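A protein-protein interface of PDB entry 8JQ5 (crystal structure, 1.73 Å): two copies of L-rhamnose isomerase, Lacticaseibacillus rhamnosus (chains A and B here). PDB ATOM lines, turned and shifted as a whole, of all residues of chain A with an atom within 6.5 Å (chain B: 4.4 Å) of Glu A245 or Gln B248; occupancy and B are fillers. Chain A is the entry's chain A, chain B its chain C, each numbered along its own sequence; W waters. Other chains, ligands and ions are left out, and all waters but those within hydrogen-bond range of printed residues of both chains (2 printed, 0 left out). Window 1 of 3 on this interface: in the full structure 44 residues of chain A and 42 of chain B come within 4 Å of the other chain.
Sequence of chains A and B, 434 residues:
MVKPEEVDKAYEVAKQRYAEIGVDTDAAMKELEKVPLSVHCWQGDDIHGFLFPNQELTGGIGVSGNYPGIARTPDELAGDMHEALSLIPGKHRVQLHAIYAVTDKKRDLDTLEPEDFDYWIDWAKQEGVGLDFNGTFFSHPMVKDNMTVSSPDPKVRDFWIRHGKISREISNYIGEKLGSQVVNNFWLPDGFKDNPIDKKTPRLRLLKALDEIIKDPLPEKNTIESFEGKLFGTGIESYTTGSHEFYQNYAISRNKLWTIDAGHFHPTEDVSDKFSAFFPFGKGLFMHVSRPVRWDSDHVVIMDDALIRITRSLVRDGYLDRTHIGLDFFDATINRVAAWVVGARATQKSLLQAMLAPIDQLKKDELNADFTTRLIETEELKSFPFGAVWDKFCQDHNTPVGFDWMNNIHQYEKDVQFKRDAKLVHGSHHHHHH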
ATOM      1  N   ARG A 203      23.948   0.107 -30.011  1.00  0.00           N
ATOM      2  CA  ARG A 203      23.887  -1.258 -29.424  1.00  0.00           C
ATOM      3  C   ARG A 203      25.272  -1.909 -29.462  1.00  0.00           C
ATOM      4  O   ARG A 203      25.584  -2.657 -28.533  1.00  0.00           O
ATOM      5  CB  ARG A 203      22.782  -2.068 -30.106  1.00  0.00           C
ATOM      6  CG  ARG A 203      21.404  -1.666 -29.599  1.00  0.00           C
ATOM      7  CD  ARG A 203      20.230  -2.175 -30.402  1.00  0.00           C
ATOM      8  NE  ARG A 203      19.022  -1.713 -29.737  1.00  0.00           N
ATOM      9  CZ  ARG A 203      17.794  -1.805 -30.224  1.00  0.00           C
ATOM     10  NH1 ARG A 203      17.578  -2.357 -31.403  1.00  0.00           N
ATOM     11  NH2 ARG A 203      16.781  -1.343 -29.513  1.00  0.00           N
ATOM     12  N   GLY A 242      19.216  -0.390 -24.860  1.00  0.00           N
ATOM     13  CA  GLY A 242      19.111  -1.670 -24.137  1.00  0.00           C
ATOM     14  C   GLY A 242      17.708  -2.239 -24.254  1.00  0.00           C
ATOM     15  O   GLY A 242      16.931  -2.089 -23.293  1.00  0.00           O
ATOM     16  N   SER A 243      17.393  -2.862 -25.393  1.00  0.00           N
ATOM     17  CA  SER A 243      16.089  -3.512 -25.677  1.00  0.00           C
ATOM     18  C   SER A 243      16.000  -4.860 -24.960  1.00  0.00           C
ATOM     19  O   SER A 243      17.049  -5.418 -24.575  1.00  0.00           O
ATOM     20  CB  SER A 243      15.859  -3.673 -27.164  1.00  0.00           C
ATOM     21  OG  SER A 243      16.701  -4.677 -27.710  1.00  0.00           O
ATOM     22  N   HIS A 244      14.789  -5.387 -24.812  1.00  0.00           N
ATOM     23  CA  HIS A 244      14.558  -6.745 -24.252  1.00  0.00           C
ATOM     24  C   HIS A 244      15.333  -7.787 -25.069  1.00  0.00           C
ATOM     25  O   HIS A 244      15.916  -8.709 -24.458  1.00  0.00           O
ATOM     26  CB  HIS A 244      13.061  -7.055 -24.174  1.00  0.00           C
ATOM     27  CG  HIS A 244      12.334  -6.096 -23.306  1.00  0.00           C
ATOM     28  ND1 HIS A 244      12.714  -5.873 -21.997  1.00  0.00           N
ATOM     29  CD2 HIS A 244      11.255  -5.315 -23.539  1.00  0.00           C
ATOM     30  CE1 HIS A 244      11.895  -4.989 -21.457  1.00  0.00           C
ATOM     31  NE2 HIS A 244      10.987  -4.634 -22.384  1.00  0.00           N
ATOM     32  N   GLU A 245      15.332  -7.671 -26.400  1.00  0.00           N
ATOM     33  CA  GLU A 245      16.011  -8.657 -27.276  1.00  0.00           C
ATOM     34  C   GLU A 245      17.512  -8.534 -27.033  1.00  0.00           C
ATOM     35  O   GLU A 245      18.171  -9.568 -26.850  1.00  0.00           O
ATOM     36  CB  GLU A 245      15.662  -8.433 -28.745  1.00  0.00           C
ATOM     37  CG  GLU A 245      14.262  -8.873 -29.106  1.00  0.00           C
ATOM     38  CD  GLU A 245      13.173  -7.887 -28.730  1.00  0.00           C
ATOM     39  OE1 GLU A 245      13.508  -6.755 -28.310  1.00  0.00           O
ATOM     40  OE2 GLU A 245      11.996  -8.256 -28.870  1.00  0.00           O
ATOM     41  N   PHE A 246      18.024  -7.305 -27.001  1.00  0.00           N
ATOM     42  CA  PHE A 246      19.462  -7.064 -26.764  1.00  0.00           C
ATOM     43  C   PHE A 246      19.877  -7.759 -25.460  1.00  0.00           C
ATOM     44  O   PHE A 246      20.877  -8.477 -25.447  1.00  0.00           O
ATOM     45  CB  PHE A 246      19.795  -5.570 -26.709  1.00  0.00           C
ATOM     46  CG  PHE A 246      21.263  -5.344 -26.473  1.00  0.00           C
ATOM     47  CD1 PHE A 246      22.137  -5.246 -27.539  1.00  0.00           C
ATOM     48  CD2 PHE A 246      21.769  -5.283 -25.185  1.00  0.00           C
ATOM     49  CE1 PHE A 246      23.496  -5.072 -27.324  1.00  0.00           C
ATOM     50  CE2 PHE A 246      23.126  -5.106 -24.970  1.00  0.00           C
ATOM     51  CZ  PHE A 246      23.986  -4.998 -26.040  1.00  0.00           C
ATOM     52  N   TYR A 247      19.129  -7.563 -24.376  1.00  0.00           N
ATOM     53  CA  TYR A 247      19.578  -8.012 -23.038  1.00  0.00           C
ATOM     54  C   TYR A 247      19.371  -9.526 -22.872  1.00  0.00           C
ATOM     55  O   TYR A 247      20.189 -10.151 -22.204  1.00  0.00           O
ATOM     56  CB  TYR A 247      18.917  -7.189 -21.941  1.00  0.00           C
ATOM     57  CG  TYR A 247      19.544  -5.837 -21.706  1.00  0.00           C
ATOM     58  CD1 TYR A 247      20.912  -5.681 -21.550  1.00  0.00           C
ATOM     59  CD2 TYR A 247      18.754  -4.711 -21.592  1.00  0.00           C
ATOM     60  CE1 TYR A 247      21.472  -4.443 -21.285  1.00  0.00           C
ATOM     61  CE2 TYR A 247      19.298  -3.465 -21.344  1.00  0.00           C
ATOM     62  CZ  TYR A 247      20.660  -3.328 -21.181  1.00  0.00           C
ATOM     63  OH  TYR A 247      21.168  -2.092 -20.913  1.00  0.00           O
ATOM     64  N   GLN A 248      18.324 -10.110 -23.454  1.00  0.00           N
ATOM     65  CA  GLN A 248      18.146 -11.581 -23.392  1.00  0.00           C
ATOM     66  C   GLN A 248      19.326 -12.202 -24.141  1.00  0.00           C
ATOM     67  O   GLN A 248      19.984 -13.126 -23.595  1.00  0.00           O
ATOM     68  CB  GLN A 248      16.802 -12.055 -23.954  1.00  0.00           C
ATOM     69  CG  GLN A 248      16.703 -13.580 -23.911  1.00  0.00           C
ATOM     70  CD  GLN A 248      15.304 -14.149 -23.978  1.00  0.00           C
ATOM     71  OE1 GLN A 248      15.107 -15.336 -23.727  1.00  0.00           O
ATOM     72  NE2 GLN A 248      14.333 -13.311 -24.328  1.00  0.00           N
ATOM     73  N   ASN A 249      19.643 -11.672 -25.321  1.00  0.00           N
ATOM     74  CA  ASN A 249      20.816 -12.162 -26.099  1.00  0.00           C
ATOM     75  C   ASN A 249      22.083 -11.983 -25.258  1.00  0.00           C
ATOM     76  O   ASN A 249      22.936 -12.914 -25.242  1.00  0.00           O
ATOM     77  CB  ASN A 249      20.939 -11.455 -27.451  1.00  0.00           C
ATOM     78  CG  ASN A 249      19.819 -11.817 -28.406  1.00  0.00           C
ATOM     79  OD1 ASN A 249      19.135 -12.830 -28.224  1.00  0.00           O
ATOM     80  ND2 ASN A 249      19.630 -11.001 -29.430  1.00  0.00           N
ATOM     81  N   TYR A 250      22.228 -10.829 -24.600  1.00  0.00           N
ATOM     82  CA  TYR A 250      23.464 -10.479 -23.855  1.00  0.00           C
ATOM     83  C   TYR A 250      23.597 -11.420 -22.651  1.00  0.00           C
ATOM     84  O   TYR A 250      24.672 -12.002 -22.451  1.00  0.00           O
ATOM     85  CB  TYR A 250      23.489  -9.006 -23.445  1.00  0.00           C
ATOM     86  CG  TYR A 250      24.812  -8.624 -22.841  1.00  0.00           C
ATOM     87  CD1 TYR A 250      25.897  -8.321 -23.645  1.00  0.00           C
ATOM     88  CD2 TYR A 250      25.013  -8.681 -21.474  1.00  0.00           C
ATOM     89  CE1 TYR A 250      27.132  -8.015 -23.099  1.00  0.00           C
ATOM     90  CE2 TYR A 250      26.247  -8.394 -20.914  1.00  0.00           C
ATOM     91  CZ  TYR A 250      27.307  -8.050 -21.728  1.00  0.00           C
ATOM     92  OH  TYR A 250      28.525  -7.768 -21.180  1.00  0.00           O
ATOM     93  N   TRP A 258      18.911 -12.164 -16.696  1.00  0.00           N
ATOM     94  CA  TRP A 258      18.052 -11.264 -17.500  1.00  0.00           C
ATOM     95  C   TRP A 258      16.971 -10.723 -16.569  1.00  0.00           C
ATOM     96  O   TRP A 258      16.373 -11.524 -15.827  1.00  0.00           O
ATOM     97  CB  TRP A 258      17.496 -12.014 -18.715  1.00  0.00           C
ATOM     98  CG  TRP A 258      16.638 -11.181 -19.613  1.00  0.00           C
ATOM     99  CD1 TRP A 258      16.845  -9.885 -19.991  1.00  0.00           C
ATOM    100  CD2 TRP A 258      15.452 -11.617 -20.298  1.00  0.00           C
ATOM    101  NE1 TRP A 258      15.830  -9.466 -20.811  1.00  0.00           N
ATOM    102  CE2 TRP A 258      14.968 -10.509 -21.024  1.00  0.00           C
ATOM    103  CE3 TRP A 258      14.737 -12.820 -20.337  1.00  0.00           C
ATOM    104  CZ2 TRP A 258      13.803 -10.576 -21.786  1.00  0.00           C
ATOM    105  CZ3 TRP A 258      13.592 -12.886 -21.097  1.00  0.00           C
ATOM    106  CH2 TRP A 258      13.133 -11.776 -21.812  1.00  0.00           C
ATOM    107  N   HIS A 266       5.223  -4.186 -24.364  1.00  0.00           N
ATOM    108  CA  HIS A 266       4.188  -3.654 -25.289  1.00  0.00           C
ATOM    109  C   HIS A 266       2.814  -3.751 -24.646  1.00  0.00           C
ATOM    110  O   HIS A 266       2.583  -4.567 -23.749  1.00  0.00           O
ATOM    111  CB  HIS A 266       4.194  -4.427 -26.610  1.00  0.00           C
ATOM    112  CG  HIS A 266       5.406  -4.172 -27.438  1.00  0.00           C
ATOM    113  ND1 HIS A 266       6.564  -4.913 -27.294  1.00  0.00           N
ATOM    114  CD2 HIS A 266       5.638  -3.270 -28.416  1.00  0.00           C
ATOM    115  CE1 HIS A 266       7.471  -4.454 -28.134  1.00  0.00           C
ATOM    116  NE2 HIS A 266       6.918  -3.451 -28.843  1.00  0.00           N
ATOM    117  N   GLU A 269       1.242  -7.286 -23.981  1.00  0.00           N
ATOM    118  CA  GLU A 269       2.373  -8.246 -23.908  1.00  0.00           C
ATOM    119  C   GLU A 269       2.331  -8.949 -22.543  1.00  0.00           C
ATOM    120  O   GLU A 269       2.154  -8.276 -21.520  1.00  0.00           O
ATOM    121  CB  GLU A 269       3.693  -7.545 -24.214  1.00  0.00           C
ATOM    122  CG  GLU A 269       4.873  -8.510 -24.321  1.00  0.00           C
ATOM    123  CD  GLU A 269       6.013  -7.984 -25.169  1.00  0.00           C
ATOM    124  OE1 GLU A 269       6.820  -8.785 -25.606  1.00  0.00           O
ATOM    125  OE2 GLU A 269       6.087  -6.768 -25.372  1.00  0.00           O
ATOM    126  N   HIS B 244       8.732 -15.842 -30.603  1.00  0.00           N
ATOM    127  CA  HIS B 244       9.830 -15.005 -31.157  1.00  0.00           C
ATOM    128  C   HIS B 244      11.098 -15.176 -30.308  1.00  0.00           C
ATOM    129  O   HIS B 244      12.187 -15.320 -30.885  1.00  0.00           O
ATOM    130  CB  HIS B 244       9.365 -13.555 -31.259  1.00  0.00           C
ATOM    131  CG  HIS B 244       8.229 -13.374 -32.204  1.00  0.00           C
ATOM    132  ND1 HIS B 244       8.275 -13.835 -33.511  1.00  0.00           N
ATOM    133  CD2 HIS B 244       7.024 -12.780 -32.039  1.00  0.00           C
ATOM    134  CE1 HIS B 244       7.140 -13.536 -34.107  1.00  0.00           C
ATOM    135  NE2 HIS B 244       6.349 -12.888 -33.224  1.00  0.00           N
ATOM    136  N   GLU B 245      10.964 -15.163 -28.983  1.00  0.00           N
ATOM    137  CA  GLU B 245      12.116 -15.298 -28.053  1.00  0.00           C
ATOM    138  C   GLU B 245      12.727 -16.682 -28.239  1.00  0.00           C
ATOM    139  O   GLU B 245      13.970 -16.793 -28.339  1.00  0.00           O
ATOM    140  CB  GLU B 245      11.675 -15.094 -26.602  1.00  0.00           C
ATOM    141  CG  GLU B 245      11.341 -13.647 -26.271  1.00  0.00           C
ATOM    142  CD  GLU B 245       9.964 -13.173 -26.705  1.00  0.00           C
ATOM    143  OE1 GLU B 245       9.728 -11.962 -26.633  1.00  0.00           O
ATOM    144  OE2 GLU B 245       9.127 -14.011 -27.104  1.00  0.00           O
ATOM    145  N   PHE B 246      11.885 -17.712 -28.282  1.00  0.00           N
ATOM    146  CA  PHE B 246      12.366 -19.103 -28.443  1.00  0.00           C
ATOM    147  C   PHE B 246      13.227 -19.166 -29.704  1.00  0.00           C
ATOM    148  O   PHE B 246      14.362 -19.637 -29.638  1.00  0.00           O
ATOM    149  CB  PHE B 246      11.228 -20.118 -28.538  1.00  0.00           C
ATOM    150  CG  PHE B 246      11.731 -21.529 -28.689  1.00  0.00           C
ATOM    151  CD1 PHE B 246      11.997 -22.307 -27.574  1.00  0.00           C
ATOM    152  CD2 PHE B 246      11.983 -22.065 -29.940  1.00  0.00           C
ATOM    153  CE1 PHE B 246      12.486 -23.596 -27.709  1.00  0.00           C
ATOM    154  CE2 PHE B 246      12.471 -23.357 -30.074  1.00  0.00           C
ATOM    155  CZ  PHE B 246      12.718 -24.119 -28.961  1.00  0.00           C
ATOM    156  N   TYR B 247      12.716 -18.660 -30.823  1.00  0.00           N
ATOM    157  CA  TYR B 247      13.385 -18.840 -32.134  1.00  0.00           C
ATOM    158  C   TYR B 247      14.618 -17.938 -32.261  1.00  0.00           C
ATOM    159  O   TYR B 247      15.560 -18.390 -32.921  1.00  0.00           O
ATOM    160  CB  TYR B 247      12.412 -18.634 -33.289  1.00  0.00           C
ATOM    161  CG  TYR B 247      11.504 -19.808 -33.534  1.00  0.00           C
ATOM    162  CD1 TYR B 247      12.005 -21.099 -33.602  1.00  0.00           C
ATOM    163  CD2 TYR B 247      10.142 -19.626 -33.703  1.00  0.00           C
ATOM    164  CE1 TYR B 247      11.176 -22.183 -33.841  1.00  0.00           C
ATOM    165  CE2 TYR B 247       9.303 -20.695 -33.954  1.00  0.00           C
ATOM    166  CZ  TYR B 247       9.822 -21.976 -34.031  1.00  0.00           C
ATOM    167  OH  TYR B 247       8.994 -23.026 -34.291  1.00  0.00           O
ATOM    168  N   GLN B 248      14.610 -16.722 -31.712  1.00  0.00           N
ATOM    169  CA  GLN B 248      15.817 -15.858 -31.737  1.00  0.00           C
ATOM    170  C   GLN B 248      16.917 -16.589 -30.950  1.00  0.00           C
ATOM    171  O   GLN B 248      18.057 -16.712 -31.466  1.00  0.00           O
ATOM    172  CB  GLN B 248      15.554 -14.446 -31.199  1.00  0.00           C
ATOM    173  CG  GLN B 248      16.820 -13.604 -31.242  1.00  0.00           C
ATOM    174  CD  GLN B 248      16.666 -12.106 -31.197  1.00  0.00           C
ATOM    175  OE1 GLN B 248      17.624 -11.384 -31.463  1.00  0.00           O
ATOM    176  NE2 GLN B 248      15.486 -11.621 -30.833  1.00  0.00           N
ATOM    177  N   ASN B 249      16.577 -17.103 -29.764  1.00  0.00           N
ATOM    178  CA  ASN B 249      17.533 -17.864 -28.916  1.00  0.00           C
ATOM    179  C   ASN B 249      18.006 -19.086 -29.703  1.00  0.00           C
ATOM    180  O   ASN B 249      19.227 -19.380 -29.686  1.00  0.00           O
ATOM    181  CB  ASN B 249      16.914 -18.260 -27.577  1.00  0.00           C
ATOM    182  CG  ASN B 249      16.640 -17.075 -26.676  1.00  0.00           C
ATOM    183  OD1 ASN B 249      17.225 -16.009 -26.852  1.00  0.00           O
ATOM    184  ND2 ASN B 249      15.771 -17.256 -25.695  1.00  0.00           N
ATOM    185  N   TYR B 250      17.082 -19.798 -30.355  1.00  0.00           N
ATOM    186  CA  TYR B 250      17.422 -21.044 -31.093  1.00  0.00           C
ATOM    187  C   TYR B 250      18.335 -20.695 -32.270  1.00  0.00           C
ATOM    188  O   TYR B 250      19.390 -21.355 -32.453  1.00  0.00           O
ATOM    189  CB  TYR B 250      16.177 -21.771 -31.596  1.00  0.00           C
ATOM    190  CG  TYR B 250      16.486 -23.141 -32.138  1.00  0.00           C
ATOM    191  CD1 TYR B 250      16.656 -24.220 -31.288  1.00  0.00           C
ATOM    192  CD2 TYR B 250      16.653 -23.351 -33.495  1.00  0.00           C
ATOM    193  CE1 TYR B 250      16.972 -25.477 -31.774  1.00  0.00           C
ATOM    194  CE2 TYR B 250      16.974 -24.601 -34.002  1.00  0.00           C
ATOM    195  CZ  TYR B 250      17.147 -25.669 -33.136  1.00  0.00           C
ATOM    196  OH  TYR B 250      17.453 -26.913 -33.621  1.00  0.00           O
ATOM    197  N   ALA B 251      17.957 -19.693 -33.070  1.00  0.00           N
ATOM    198  CA  ALA B 251      18.758 -19.291 -34.253  1.00  0.00           C
ATOM    199  C   ALA B 251      20.187 -18.956 -33.821  1.00  0.00           C
ATOM    200  O   ALA B 251      21.132 -19.414 -34.489  1.00  0.00           O
ATOM    201  CB  ALA B 251      18.144 -18.126 -34.977  1.00  0.00           C
ATOM    202  N   ILE B 252      20.345 -18.133 -32.786  1.00  0.00           N
ATOM    203  CA  ILE B 252      21.694 -17.694 -32.326  1.00  0.00           C
ATOM    204  C   ILE B 252      22.475 -18.907 -31.822  1.00  0.00           C
ATOM    205  O   ILE B 252      23.677 -19.047 -32.202  1.00  0.00           O
ATOM    206  CB  ILE B 252      21.569 -16.597 -31.255  1.00  0.00           C
ATOM    207  CG1 ILE B 252      21.041 -15.308 -31.892  1.00  0.00           C
ATOM    208  CG2 ILE B 252      22.915 -16.408 -30.554  1.00  0.00           C
ATOM    209  CD1 ILE B 252      20.560 -14.256 -30.919  1.00  0.00           C
ATOM    210  N   TRP B 258      17.009 -16.393 -38.308  1.00  0.00           N
ATOM    211  CA  TRP B 258      15.763 -16.038 -37.589  1.00  0.00           C
ATOM    212  C   TRP B 258      14.788 -15.375 -38.574  1.00  0.00           C
ATOM    213  O   TRP B 258      15.206 -14.454 -39.299  1.00  0.00           O
ATOM    214  CB  TRP B 258      16.096 -15.151 -36.381  1.00  0.00           C
ATOM    215  CG  TRP B 258      14.903 -14.769 -35.558  1.00  0.00           C
ATOM    216  CD1 TRP B 258      13.843 -15.558 -35.225  1.00  0.00           C
ATOM    217  CD2 TRP B 258      14.672 -13.499 -34.926  1.00  0.00           C
ATOM    218  NE1 TRP B 258      12.946 -14.850 -34.467  1.00  0.00           N
ATOM    219  CE2 TRP B 258      13.431 -13.589 -34.259  1.00  0.00           C
ATOM    220  CE3 TRP B 258      15.373 -12.293 -34.884  1.00  0.00           C
ATOM    221  CZ2 TRP B 258      12.887 -12.515 -33.560  1.00  0.00           C
ATOM    222  CZ3 TRP B 258      14.837 -11.237 -34.185  1.00  0.00           C
ATOM    223  CH2 TRP B 258      13.604 -11.342 -33.547  1.00  0.00           C
ATOM    224  N   LYS B 274      14.252  -4.854 -34.105  1.00  0.00           N
ATOM    225  CA  LYS B 274      14.873  -6.152 -33.713  1.00  0.00           C
ATOM    226  C   LYS B 274      16.235  -6.330 -34.384  1.00  0.00           C
ATOM    227  O   LYS B 274      17.079  -6.978 -33.762  1.00  0.00           O
ATOM    228  CB  LYS B 274      13.985  -7.350 -34.061  1.00  0.00           C
ATOM    229  CG  LYS B 274      12.519  -7.190 -33.690  1.00  0.00           C
ATOM    230  CD  LYS B 274      12.263  -7.062 -32.209  1.00  0.00           C
ATOM    231  CE  LYS B 274      10.778  -7.064 -31.892  1.00  0.00           C
ATOM    232  NZ  LYS B 274      10.501  -6.575 -30.524  1.00  0.00           N
ATOM    233  N   ALA B 277      19.426  -5.455 -32.534  1.00  0.00           N
ATOM    234  CA  ALA B 277      19.482  -6.194 -31.257  1.00  0.00           C
ATOM    235  C   ALA B 277      19.885  -7.645 -31.545  1.00  0.00           C
ATOM    236  O   ALA B 277      20.394  -8.310 -30.628  1.00  0.00           O
ATOM    237  CB  ALA B 277      18.154  -6.109 -30.538  1.00  0.00           C
ATOM    238  N   PHE B 278      19.698  -8.100 -32.787  1.00  0.00           N
ATOM    239  CA  PHE B 278      20.013  -9.478 -33.249  1.00  0.00           C
ATOM    240  C   PHE B 278      21.454  -9.560 -33.771  1.00  0.00           C
ATOM    241  O   PHE B 278      22.174 -10.493 -33.385  1.00  0.00           O
ATOM    242  CB  PHE B 278      19.038  -9.928 -34.343  1.00  0.00           C
ATOM    243  CG  PHE B 278      19.397 -11.233 -35.013  1.00  0.00           C
ATOM    244  CD1 PHE B 278      19.066 -12.446 -34.429  1.00  0.00           C
ATOM    245  CD2 PHE B 278      20.072 -11.247 -36.224  1.00  0.00           C
ATOM    246  CE1 PHE B 278      19.389 -13.644 -35.046  1.00  0.00           C
ATOM    247  CE2 PHE B 278      20.394 -12.446 -36.839  1.00  0.00           C
ATOM    248  CZ  PHE B 278      20.052 -13.638 -36.249  1.00  0.00           C
HETATM  249  O   HOH W   1      16.609 -13.432 -27.595  1.00  0.00           O
HETATM  250  O   HOH W   2      19.913 -15.449 -27.472  1.00  0.00           O
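NZ of Lys B274 is in salt-bridge range of OE2 of Glu A245 (2.8 Å). The side-chain amide oxygen (OE1) of Gln A248 sits at hydrogen-bond distance from the side-chain amide nitrogen (ND2) of Asn B249. OE1 of Gln B248 is in hydrogen-bond range of ND2 of Asn A249 (2.9 Å). The backbone carbonyl oxygen (O) of Ala B277 is in hydrogen-bond range of the side-chain amide nitrogen (ND2) of Asn A249, at 3.0 Å.
The side-chain hydroxyl of Ser A243 is in hydrogen-bond range of the backbone NH of Phe A246 (3.0 Å). The backbone carbonyl oxygen (O) of Glu A245 lies close to the side-chain amide nitrogen (ND2) of Asn A249, 3.3 Å away. ND2 of Asn B249 sits close to O of Glu B245, at 3.2 Å.
Ala B277 touches Arg A203. OG of Ser A243 touches CB of Ala B277, 3.5 Å away. Glu A245 touches Gln B248. Glu A245 touches Ala B277. CB of Ala B277 touches N of Phe A246, 3.7 Å away. Glu B245 touches Gln A248. Asn A249 touches Asn B249 (OD1 to OD1, 3.95 Å). CD1 of Ile B252 touches OD1 of Asn A249, 3.4 Å away.
Glu A245 touches just these residues of chain B: Gln B248 (3.5 Å), Lys B274 (2.8 Å) and Ala B277 (3.9 Å). Of the printed residues of chain B, Phe A246 touches Ala B277 (3.7 Å). His A266 touches none of the printed residues of chain B. Gln B248 touches just these residues of chain A: Glu A245 (3.5 Å) and Asn A249 (2.9 Å). Tyr B250 touches none of the printed residues of chain A. Printed residues of chain A within 4 Å of Ala B277: Arg A203, Ser A243, Glu A245, Phe A246 and Asn A249. The nearest printed residue of chain B that does not touch Glu A245 is Glu B245 (4.9 Å).
Along chain A the printed residues that touch a printed residue of chain B span positions 203 to 249. Of the 13 printed residues of chain B, 6 touch a printed residue of chain A. Hydrophobic or aromatic side chains of chain B that line the printed part of chain A: Ile B252 and Ala B277. Among the printed residues, Asp or Glu carboxylates within 4 Å of a Lys or Arg side-chain nitrogen of the other chain: Glu A245 with Lys B274.
Glu A245 touches Gln B248, and with the chains exchanged Gln A248 touches Glu B245. Gln A248 touches Asn B249, and with the chains exchanged Asn A249 touches Gln B248. Asn B249 touches its own counterpart, Asn A249. 8 positions are printed for both chains. Of the 12 pairs that touch across the chains among the printed residues, 5 have their exchanged pair printed and touching as well.
Water W1 bridges the side-chain amide oxygen of Asn A249 and the side-chain amide oxygen of Asn B249. Water W2 bridges the side-chain amide oxygen (OD1) of Asn B249 (2.8 Å) and the side-chain amide oxygen (OD1) of Asn A249 (2.8 Å).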
